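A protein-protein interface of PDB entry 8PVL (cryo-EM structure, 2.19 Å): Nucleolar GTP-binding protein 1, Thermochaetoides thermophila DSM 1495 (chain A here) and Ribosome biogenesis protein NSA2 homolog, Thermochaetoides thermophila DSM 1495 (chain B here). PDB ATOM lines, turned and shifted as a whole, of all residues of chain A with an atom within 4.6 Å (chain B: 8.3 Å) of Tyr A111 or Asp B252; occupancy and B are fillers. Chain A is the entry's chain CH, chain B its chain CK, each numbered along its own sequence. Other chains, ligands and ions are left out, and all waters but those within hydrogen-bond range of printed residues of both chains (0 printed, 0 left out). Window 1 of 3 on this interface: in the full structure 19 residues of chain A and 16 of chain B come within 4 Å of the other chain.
O of Asp B252 is in hydrogen-bond range of OH of Tyr A111 (2.6 Å).
Among the printed residues, merely in contact across the chains: Leu A127 with Asn B251, Leu A127 with Glu B250, Leu A114 with Gly B176, Tyr A111 with Gly B253, Arg A113 with Gly B176, Leu A114 with Gly B253, Ala A130 with Asp B252, Leu A114 with Tyr B179 and Leu A127 with Gly B253.
Tyr A111 touches just these residues of chain B: Asp B252 (2.6 Å) and Gly B253 (3.6 Å). Of the printed residues of chain A, Gly B176 touches Arg A113 and Leu A114. Of the printed residues of chain A, Tyr B179 touches Leu A114 (3.8 Å). Printed residues of chain A within 4 Å of Glu B250: Leu A127 (3.5 Å). Of the printed residues of chain A, Asn B251 touches Leu A127 (3.4 Å). Of chain A, only Tyr A111 and Ala A130 come within 4 Å of Asp B252. Printed residues of chain A within 4 Å of Gly B253: Tyr A111, Leu A114 and Leu A127. The nearest residue of chain A that does not touch Asp B252 is Leu A127 (4.4 Å).
The side-chain carboxylate of Asp A110 lies within salt-bridge range of the guanidinium group of Arg A113, 3.1 Å away. The guanidinium group of Arg A134 sits at hydrogen-bond distance from the side-chain hydroxyl of Tyr A111 (3.2 Å). O of Gly B253 lies within hydrogen-bond range of OH of Tyr B179, 2.9 Å away. The side-chain amide nitrogen (ND2) of Asn B247 is in hydrogen-bond range of the side-chain carboxylate (OD2) of Asp B252 (3.1 Å).
Along chain A the printed residues that touch a printed residue of chain B span positions 111 to 130. Among the printed residues, no Asp or Glu carboxylate lies within 4 Å of a Lys or Arg side-chain nitrogen of the other chain.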
ATOM      1  N   ILE A 107      -8.695 -18.788  21.624  1.00  0.00           N
ATOM      2  CA  ILE A 107      -8.091 -18.642  20.300  1.00  0.00           C
ATOM      3  C   ILE A 107      -8.079 -19.978  19.568  1.00  0.00           C
ATOM      4  O   ILE A 107      -8.391 -20.054  18.369  1.00  0.00           O
ATOM      5  CB  ILE A 107      -6.676 -18.045  20.435  1.00  0.00           C
ATOM      6  CG1 ILE A 107      -6.750 -16.524  20.550  1.00  0.00           C
ATOM      7  CG2 ILE A 107      -5.775 -18.440  19.271  1.00  0.00           C
ATOM      8  CD1 ILE A 107      -5.425 -15.884  20.833  1.00  0.00           C
ATOM      9  N   SER A 108      -7.734 -21.052  20.286  1.00  0.00           N
ATOM     10  CA  SER A 108      -7.711 -22.382  19.687  1.00  0.00           C
ATOM     11  C   SER A 108      -9.089 -22.810  19.207  1.00  0.00           C
ATOM     12  O   SER A 108      -9.224 -23.358  18.106  1.00  0.00           O
ATOM     13  CB  SER A 108      -7.175 -23.392  20.689  1.00  0.00           C
ATOM     14  OG  SER A 108      -7.197 -24.704  20.161  1.00  0.00           O
ATOM     15  N   ARG A 109     -10.124 -22.567  20.020  1.00  0.00           N
ATOM     16  CA  ARG A 109     -11.480 -22.927  19.609  1.00  0.00           C
ATOM     17  C   ARG A 109     -11.911 -22.153  18.367  1.00  0.00           C
ATOM     18  O   ARG A 109     -12.484 -22.735  17.432  1.00  0.00           O
ATOM     19  CB  ARG A 109     -12.458 -22.693  20.758  1.00  0.00           C
ATOM     20  CG  ARG A 109     -12.390 -23.748  21.846  1.00  0.00           C
ATOM     21  CD  ARG A 109     -13.628 -23.717  22.724  1.00  0.00           C
ATOM     22  NE  ARG A 109     -13.973 -22.356  23.115  1.00  0.00           N
ATOM     23  CZ  ARG A 109     -13.531 -21.759  24.212  1.00  0.00           C
ATOM     24  NH1 ARG A 109     -12.736 -22.384  25.066  1.00  0.00           N
ATOM     25  NH2 ARG A 109     -13.891 -20.503  24.457  1.00  0.00           N
ATOM     26  N   ASP A 110     -11.607 -20.849  18.325  1.00  0.00           N
ATOM     27  CA  ASP A 110     -11.978 -20.031  17.170  1.00  0.00           C
ATOM     28  C   ASP A 110     -11.293 -20.516  15.895  1.00  0.00           C
ATOM     29  O   ASP A 110     -11.932 -20.657  14.843  1.00  0.00           O
ATOM     30  CB  ASP A 110     -11.633 -18.566  17.432  1.00  0.00           C
ATOM     31  CG  ASP A 110     -12.530 -17.930  18.473  1.00  0.00           C
ATOM     32  OD1 ASP A 110     -13.597 -18.504  18.774  1.00  0.00           O
ATOM     33  OD2 ASP A 110     -12.169 -16.851  18.989  1.00  0.00           O
ATOM     34  N   TYR A 111      -9.993 -20.801  15.973  1.00  0.00           N
ATOM     35  CA  TYR A 111      -9.287 -21.176  14.754  1.00  0.00           C
ATOM     36  C   TYR A 111      -9.572 -22.610  14.325  1.00  0.00           C
ATOM     37  O   TYR A 111      -9.524 -22.904  13.128  1.00  0.00           O
ATOM     38  CB  TYR A 111      -7.793 -20.922  14.913  1.00  0.00           C
ATOM     39  CG  TYR A 111      -7.460 -19.477  14.636  1.00  0.00           C
ATOM     40  CD1 TYR A 111      -7.275 -19.028  13.337  1.00  0.00           C
ATOM     41  CD2 TYR A 111      -7.378 -18.554  15.668  1.00  0.00           C
ATOM     42  CE1 TYR A 111      -6.990 -17.707  13.076  1.00  0.00           C
ATOM     43  CE2 TYR A 111      -7.094 -17.230  15.416  1.00  0.00           C
ATOM     44  CZ  TYR A 111      -6.901 -16.812  14.119  1.00  0.00           C
ATOM     45  OH  TYR A 111      -6.617 -15.493  13.864  1.00  0.00           O
ATOM     46  N   VAL A 112      -9.910 -23.503  15.261  1.00  0.00           N
ATOM     47  CA  VAL A 112     -10.397 -24.827  14.876  1.00  0.00           C
ATOM     48  C   VAL A 112     -11.729 -24.707  14.140  1.00  0.00           C
ATOM     49  O   VAL A 112     -11.960 -25.369  13.112  1.00  0.00           O
ATOM     50  CB  VAL A 112     -10.495 -25.733  16.120  1.00  0.00           C
ATOM     51  CG1 VAL A 112     -11.449 -26.894  15.895  1.00  0.00           C
ATOM     52  CG2 VAL A 112      -9.119 -26.249  16.500  1.00  0.00           C
ATOM     53  N   ARG A 113     -12.608 -23.821  14.628  1.00  0.00           N
ATOM     54  CA  ARG A 113     -13.884 -23.591  13.958  1.00  0.00           C
ATOM     55  C   ARG A 113     -13.690 -23.025  12.553  1.00  0.00           C
ATOM     56  O   ARG A 113     -14.437 -23.368  11.632  1.00  0.00           O
ATOM     57  CB  ARG A 113     -14.752 -22.657  14.802  1.00  0.00           C
ATOM     58  CG  ARG A 113     -16.237 -22.764  14.517  1.00  0.00           C
ATOM     59  CD  ARG A 113     -17.048 -21.765  15.328  1.00  0.00           C
ATOM     60  NE  ARG A 113     -16.908 -21.946  16.769  1.00  0.00           N
ATOM     61  CZ  ARG A 113     -16.262 -21.108  17.566  1.00  0.00           C
ATOM     62  NH1 ARG A 113     -15.666 -20.026  17.093  1.00  0.00           N
ATOM     63  NH2 ARG A 113     -16.209 -21.363  18.870  1.00  0.00           N
ATOM     64  N   LEU A 114     -12.693 -22.153  12.370  1.00  0.00           N
ATOM     65  CA  LEU A 114     -12.417 -21.628  11.030  1.00  0.00           C
ATOM     66  C   LEU A 114     -11.798 -22.688  10.119  1.00  0.00           C
ATOM     67  O   LEU A 114     -12.098 -22.742   8.914  1.00  0.00           O
ATOM     68  CB  LEU A 114     -11.504 -20.409  11.121  1.00  0.00           C
ATOM     69  CG  LEU A 114     -12.079 -19.206  11.865  1.00  0.00           C
ATOM     70  CD1 LEU A 114     -11.027 -18.130  12.004  1.00  0.00           C
ATOM     71  CD2 LEU A 114     -13.311 -18.674  11.159  1.00  0.00           C
ATOM     72  N   LEU A 115     -10.922 -23.532  10.671  1.00  0.00           N
ATOM     73  CA  LEU A 115     -10.316 -24.607   9.895  1.00  0.00           C
ATOM     74  C   LEU A 115     -11.333 -25.645   9.453  1.00  0.00           C
ATOM     75  O   LEU A 115     -11.072 -26.371   8.489  1.00  0.00           O
ATOM     76  CB  LEU A 115      -9.206 -25.281  10.699  1.00  0.00           C
ATOM     77  CG  LEU A 115      -7.872 -24.542  10.717  1.00  0.00           C
ATOM     78  CD1 LEU A 115      -6.884 -25.240  11.631  1.00  0.00           C
ATOM     79  CD2 LEU A 115      -7.320 -24.425   9.312  1.00  0.00           C
ATOM     80  N   LEU A 127      -4.253 -19.859   8.485  1.00  0.00           N
ATOM     81  CA  LEU A 127      -5.040 -19.890   9.717  1.00  0.00           C
ATOM     82  C   LEU A 127      -4.257 -20.511  10.872  1.00  0.00           C
ATOM     83  O   LEU A 127      -4.311 -20.010  12.005  1.00  0.00           O
ATOM     84  CB  LEU A 127      -6.347 -20.647   9.488  1.00  0.00           C
ATOM     85  CG  LEU A 127      -7.445 -19.902   8.730  1.00  0.00           C
ATOM     86  CD1 LEU A 127      -8.661 -20.790   8.539  1.00  0.00           C
ATOM     87  CD2 LEU A 127      -7.823 -18.622   9.454  1.00  0.00           C
ATOM     88  N   ALA A 130      -1.671 -18.021  11.979  1.00  0.00           N
ATOM     89  CA  ALA A 130      -2.323 -16.953  12.730  1.00  0.00           C
ATOM     90  C   ALA A 130      -2.625 -17.378  14.161  1.00  0.00           C
ATOM     91  O   ALA A 130      -2.372 -16.619  15.107  1.00  0.00           O
ATOM     92  CB  ALA A 130      -3.605 -16.520  12.021  1.00  0.00           C
ATOM     93  N   ALA A 131      -3.148 -18.597  14.335  1.00  0.00           N
ATOM     94  CA  ALA A 131      -3.436 -19.107  15.673  1.00  0.00           C
ATOM     95  C   ALA A 131      -2.169 -19.200  16.517  1.00  0.00           C
ATOM     96  O   ALA A 131      -2.125 -18.697  17.648  1.00  0.00           O
ATOM     97  CB  ALA A 131      -4.117 -20.472  15.578  1.00  0.00           C
ATOM     98  N   ARG A 134      -0.751 -15.748  17.434  1.00  0.00           N
ATOM     99  CA  ARG A 134      -1.520 -15.070  18.473  1.00  0.00           C
ATOM    100  C   ARG A 134      -1.247 -15.669  19.850  1.00  0.00           C
ATOM    101  O   ARG A 134      -1.156 -14.932  20.844  1.00  0.00           O
ATOM    102  CB  ARG A 134      -3.005 -15.107  18.125  1.00  0.00           C
ATOM    103  CG  ARG A 134      -3.361 -14.081  17.063  1.00  0.00           C
ATOM    104  CD  ARG A 134      -4.801 -14.147  16.599  1.00  0.00           C
ATOM    105  NE  ARG A 134      -5.723 -13.576  17.570  1.00  0.00           N
ATOM    106  CZ  ARG A 134      -6.984 -13.267  17.310  1.00  0.00           C
ATOM    107  NH1 ARG A 134      -7.498 -13.415  16.101  1.00  0.00           N
ATOM    108  NH2 ARG A 134      -7.750 -12.795  18.288  1.00  0.00           N
ATOM    109  N   PRO B 154     -15.703 -14.919   5.226  1.00  0.00           N
ATOM    110  CA  PRO B 154     -16.439 -14.356   6.366  1.00  0.00           C
ATOM    111  C   PRO B 154     -17.550 -13.415   5.925  1.00  0.00           C
ATOM    112  O   PRO B 154     -17.455 -12.740   4.900  1.00  0.00           O
ATOM    113  CB  PRO B 154     -15.357 -13.604   7.148  1.00  0.00           C
ATOM    114  CG  PRO B 154     -14.101 -14.277   6.786  1.00  0.00           C
ATOM    115  CD  PRO B 154     -14.255 -14.681   5.356  1.00  0.00           C
ATOM    116  N   GLY B 176     -20.040 -20.131  12.222  1.00  0.00           N
ATOM    117  CA  GLY B 176     -18.656 -19.938  12.614  1.00  0.00           C
ATOM    118  C   GLY B 176     -17.870 -18.994  11.732  1.00  0.00           C
ATOM    119  O   GLY B 176     -16.719 -18.690  12.059  1.00  0.00           O
ATOM    120  N   TYR B 179     -18.996 -12.527  11.514  1.00  0.00           N
ATOM    121  CA  TYR B 179     -18.264 -11.558  12.313  1.00  0.00           C
ATOM    122  C   TYR B 179     -19.158 -10.378  12.664  1.00  0.00           C
ATOM    123  O   TYR B 179     -20.130 -10.076  11.969  1.00  0.00           O
ATOM    124  CB  TYR B 179     -17.012 -11.059  11.580  1.00  0.00           C
ATOM    125  CG  TYR B 179     -15.873 -12.045  11.593  1.00  0.00           C
ATOM    126  CD1 TYR B 179     -15.819 -13.079  10.672  1.00  0.00           C
ATOM    127  CD2 TYR B 179     -14.856 -11.947  12.531  1.00  0.00           C
ATOM    128  CE1 TYR B 179     -14.783 -13.986  10.681  1.00  0.00           C
ATOM    129  CE2 TYR B 179     -13.812 -12.850  12.546  1.00  0.00           C
ATOM    130  CZ  TYR B 179     -13.783 -13.868  11.618  1.00  0.00           C
ATOM    131  OH  TYR B 179     -12.751 -14.774  11.623  1.00  0.00           O
ATOM    132  N   THR B 246      -8.620  -3.943   5.002  1.00  0.00           N
ATOM    133  CA  THR B 246      -7.267  -3.895   4.472  1.00  0.00           C
ATOM    134  C   THR B 246      -6.534  -5.229   4.528  1.00  0.00           C
ATOM    135  O   THR B 246      -5.369  -5.289   4.128  1.00  0.00           O
ATOM    136  CB  THR B 246      -6.446  -2.838   5.221  1.00  0.00           C
ATOM    137  OG1 THR B 246      -6.595  -3.027   6.632  1.00  0.00           O
ATOM    138  CG2 THR B 246      -6.915  -1.446   4.850  1.00  0.00           C
ATOM    139  N   ASN B 247      -7.172  -6.294   5.003  1.00  0.00           N
ATOM    140  CA  ASN B 247      -6.513  -7.585   5.130  1.00  0.00           C
ATOM    141  C   ASN B 247      -7.354  -8.661   4.454  1.00  0.00           C
ATOM    142  O   ASN B 247      -8.377  -8.379   3.826  1.00  0.00           O
ATOM    143  CB  ASN B 247      -6.259  -7.931   6.603  1.00  0.00           C
ATOM    144  CG  ASN B 247      -7.526  -8.294   7.351  1.00  0.00           C
ATOM    145  OD1 ASN B 247      -8.576  -7.687   7.150  1.00  0.00           O
ATOM    146  ND2 ASN B 247      -7.430  -9.284   8.226  1.00  0.00           N
ATOM    147  N   ASN B 248      -6.903  -9.908   4.585  1.00  0.00           N
ATOM    148  CA  ASN B 248      -7.626 -11.076   4.103  1.00  0.00           C
ATOM    149  C   ASN B 248      -8.199 -11.826   5.301  1.00  0.00           C
ATOM    150  O   ASN B 248      -7.500 -12.642   5.920  1.00  0.00           O
ATOM    151  CB  ASN B 248      -6.710 -11.979   3.274  1.00  0.00           C
ATOM    152  CG  ASN B 248      -6.362 -11.378   1.927  1.00  0.00           C
ATOM    153  OD1 ASN B 248      -7.226 -11.203   1.071  1.00  0.00           O
ATOM    154  ND2 ASN B 248      -5.091 -11.052   1.737  1.00  0.00           N
ATOM    155  N   PRO B 249      -9.457 -11.554   5.664  1.00  0.00           N
ATOM    156  CA  PRO B 249     -10.004 -12.118   6.908  1.00  0.00           C
ATOM    157  C   PRO B 249     -10.156 -13.628   6.891  1.00  0.00           C
ATOM    158  O   PRO B 249     -10.058 -14.249   7.955  1.00  0.00           O
ATOM    159  CB  PRO B 249     -11.365 -11.417   7.039  1.00  0.00           C
ATOM    160  CG  PRO B 249     -11.256 -10.206   6.170  1.00  0.00           C
ATOM    161  CD  PRO B 249     -10.407 -10.632   5.025  1.00  0.00           C
ATOM    162  N   GLU B 250     -10.377 -14.237   5.724  1.00  0.00           N
ATOM    163  CA  GLU B 250     -10.494 -15.691   5.665  1.00  0.00           C
ATOM    164  C   GLU B 250      -9.162 -16.372   5.947  1.00  0.00           C
ATOM    165  O   GLU B 250      -9.140 -17.525   6.393  1.00  0.00           O
ATOM    166  CB  GLU B 250     -11.054 -16.123   4.306  1.00  0.00           C
ATOM    167  CG  GLU B 250     -10.065 -16.097   3.153  1.00  0.00           C
ATOM    168  CD  GLU B 250      -9.919 -14.723   2.525  1.00  0.00           C
ATOM    169  OE1 GLU B 250     -10.650 -13.795   2.930  1.00  0.00           O
ATOM    170  OE2 GLU B 250      -9.068 -14.572   1.625  1.00  0.00           O
ATOM    171  N   ASN B 251      -8.050 -15.679   5.713  1.00  0.00           N
ATOM    172  CA  ASN B 251      -6.735 -16.201   6.052  1.00  0.00           C
ATOM    173  C   ASN B 251      -6.294 -15.800   7.450  1.00  0.00           C
ATOM    174  O   ASN B 251      -5.532 -16.536   8.086  1.00  0.00           O
ATOM    175  CB  ASN B 251      -5.694 -15.716   5.041  1.00  0.00           C
ATOM    176  CG  ASN B 251      -5.913 -16.287   3.658  1.00  0.00           C
ATOM    177  OD1 ASN B 251      -6.681 -17.230   3.477  1.00  0.00           O
ATOM    178  ND2 ASN B 251      -5.237 -15.717   2.671  1.00  0.00           N
ATOM    179  N   ASP B 252      -6.763 -14.656   7.946  1.00  0.00           N
ATOM    180  CA  ASP B 252      -6.243 -14.101   9.187  1.00  0.00           C
ATOM    181  C   ASP B 252      -7.088 -14.417  10.414  1.00  0.00           C
ATOM    182  O   ASP B 252      -6.570 -14.349  11.533  1.00  0.00           O
ATOM    183  CB  ASP B 252      -6.101 -12.582   9.056  1.00  0.00           C
ATOM    184  CG  ASP B 252      -4.901 -12.188   8.230  1.00  0.00           C
ATOM    185  OD1 ASP B 252      -4.005 -13.037   8.052  1.00  0.00           O
ATOM    186  OD2 ASP B 252      -4.858 -11.038   7.747  1.00  0.00           O
ATOM    187  N   GLY B 253      -8.361 -14.756  10.242  1.00  0.00           N
ATOM    188  CA  GLY B 253      -9.225 -14.987  11.379  1.00  0.00           C
ATOM    189  C   GLY B 253      -9.758 -13.740  12.042  1.00  0.00           C
ATOM    190  O   GLY B 253     -10.390 -13.842  13.098  1.00  0.00           O
ATOM    191  N   CYS B 254      -9.524 -12.567  11.458  1.00  0.00           N
ATOM    192  CA  CYS B 254      -9.978 -11.309  12.030  1.00  0.00           C
ATOM    193  C   CYS B 254     -10.170 -10.309  10.900  1.00  0.00           C
ATOM    194  O   CYS B 254      -9.691 -10.506   9.781  1.00  0.00           O
ATOM    195  CB  CYS B 254      -8.988 -10.775  13.068  1.00  0.00           C
ATOM    196  SG  CYS B 254      -7.397 -10.268  12.382  1.00  0.00           S
ATOM    197  N   VAL B 255     -10.872  -9.224  11.203  1.00  0.00           N
ATOM    198  CA  VAL B 255     -11.149  -8.170  10.235  1.00  0.00           C
ATOM    199  C   VAL B 255     -10.342  -6.942  10.628  1.00  0.00           C
ATOM    200  O   VAL B 255     -10.498  -6.416  11.736  1.00  0.00           O
ATOM    201  CB  VAL B 255     -12.648  -7.845  10.160  1.00  0.00           C
ATOM    202  CG1 VAL B 255     -12.899  -6.752   9.139  1.00  0.00           C
ATOM    203  CG2 VAL B 255     -13.442  -9.092   9.817  1.00  0.00           C
ATOM    204  N   ASN B 256      -9.470  -6.499   9.727  1.00  0.00           N
ATOM    205  CA  ASN B 256      -8.703  -5.272   9.888  1.00  0.00           C
ATOM    206  C   ASN B 256      -9.221  -4.241   8.897  1.00  0.00           C
ATOM    207  O   ASN B 256      -9.382  -4.545   7.714  1.00  0.00           O
ATOM    208  CB  ASN B 256      -7.210  -5.516   9.657  1.00  0.00           C
ATOM    209  CG  ASN B 256      -6.576  -6.347  10.751  1.00  0.00           C
ATOM    210  OD1 ASN B 256      -6.974  -6.274  11.910  1.00  0.00           O
ATOM    211  ND2 ASN B 256      -5.581  -7.140  10.387  1.00  0.00           N
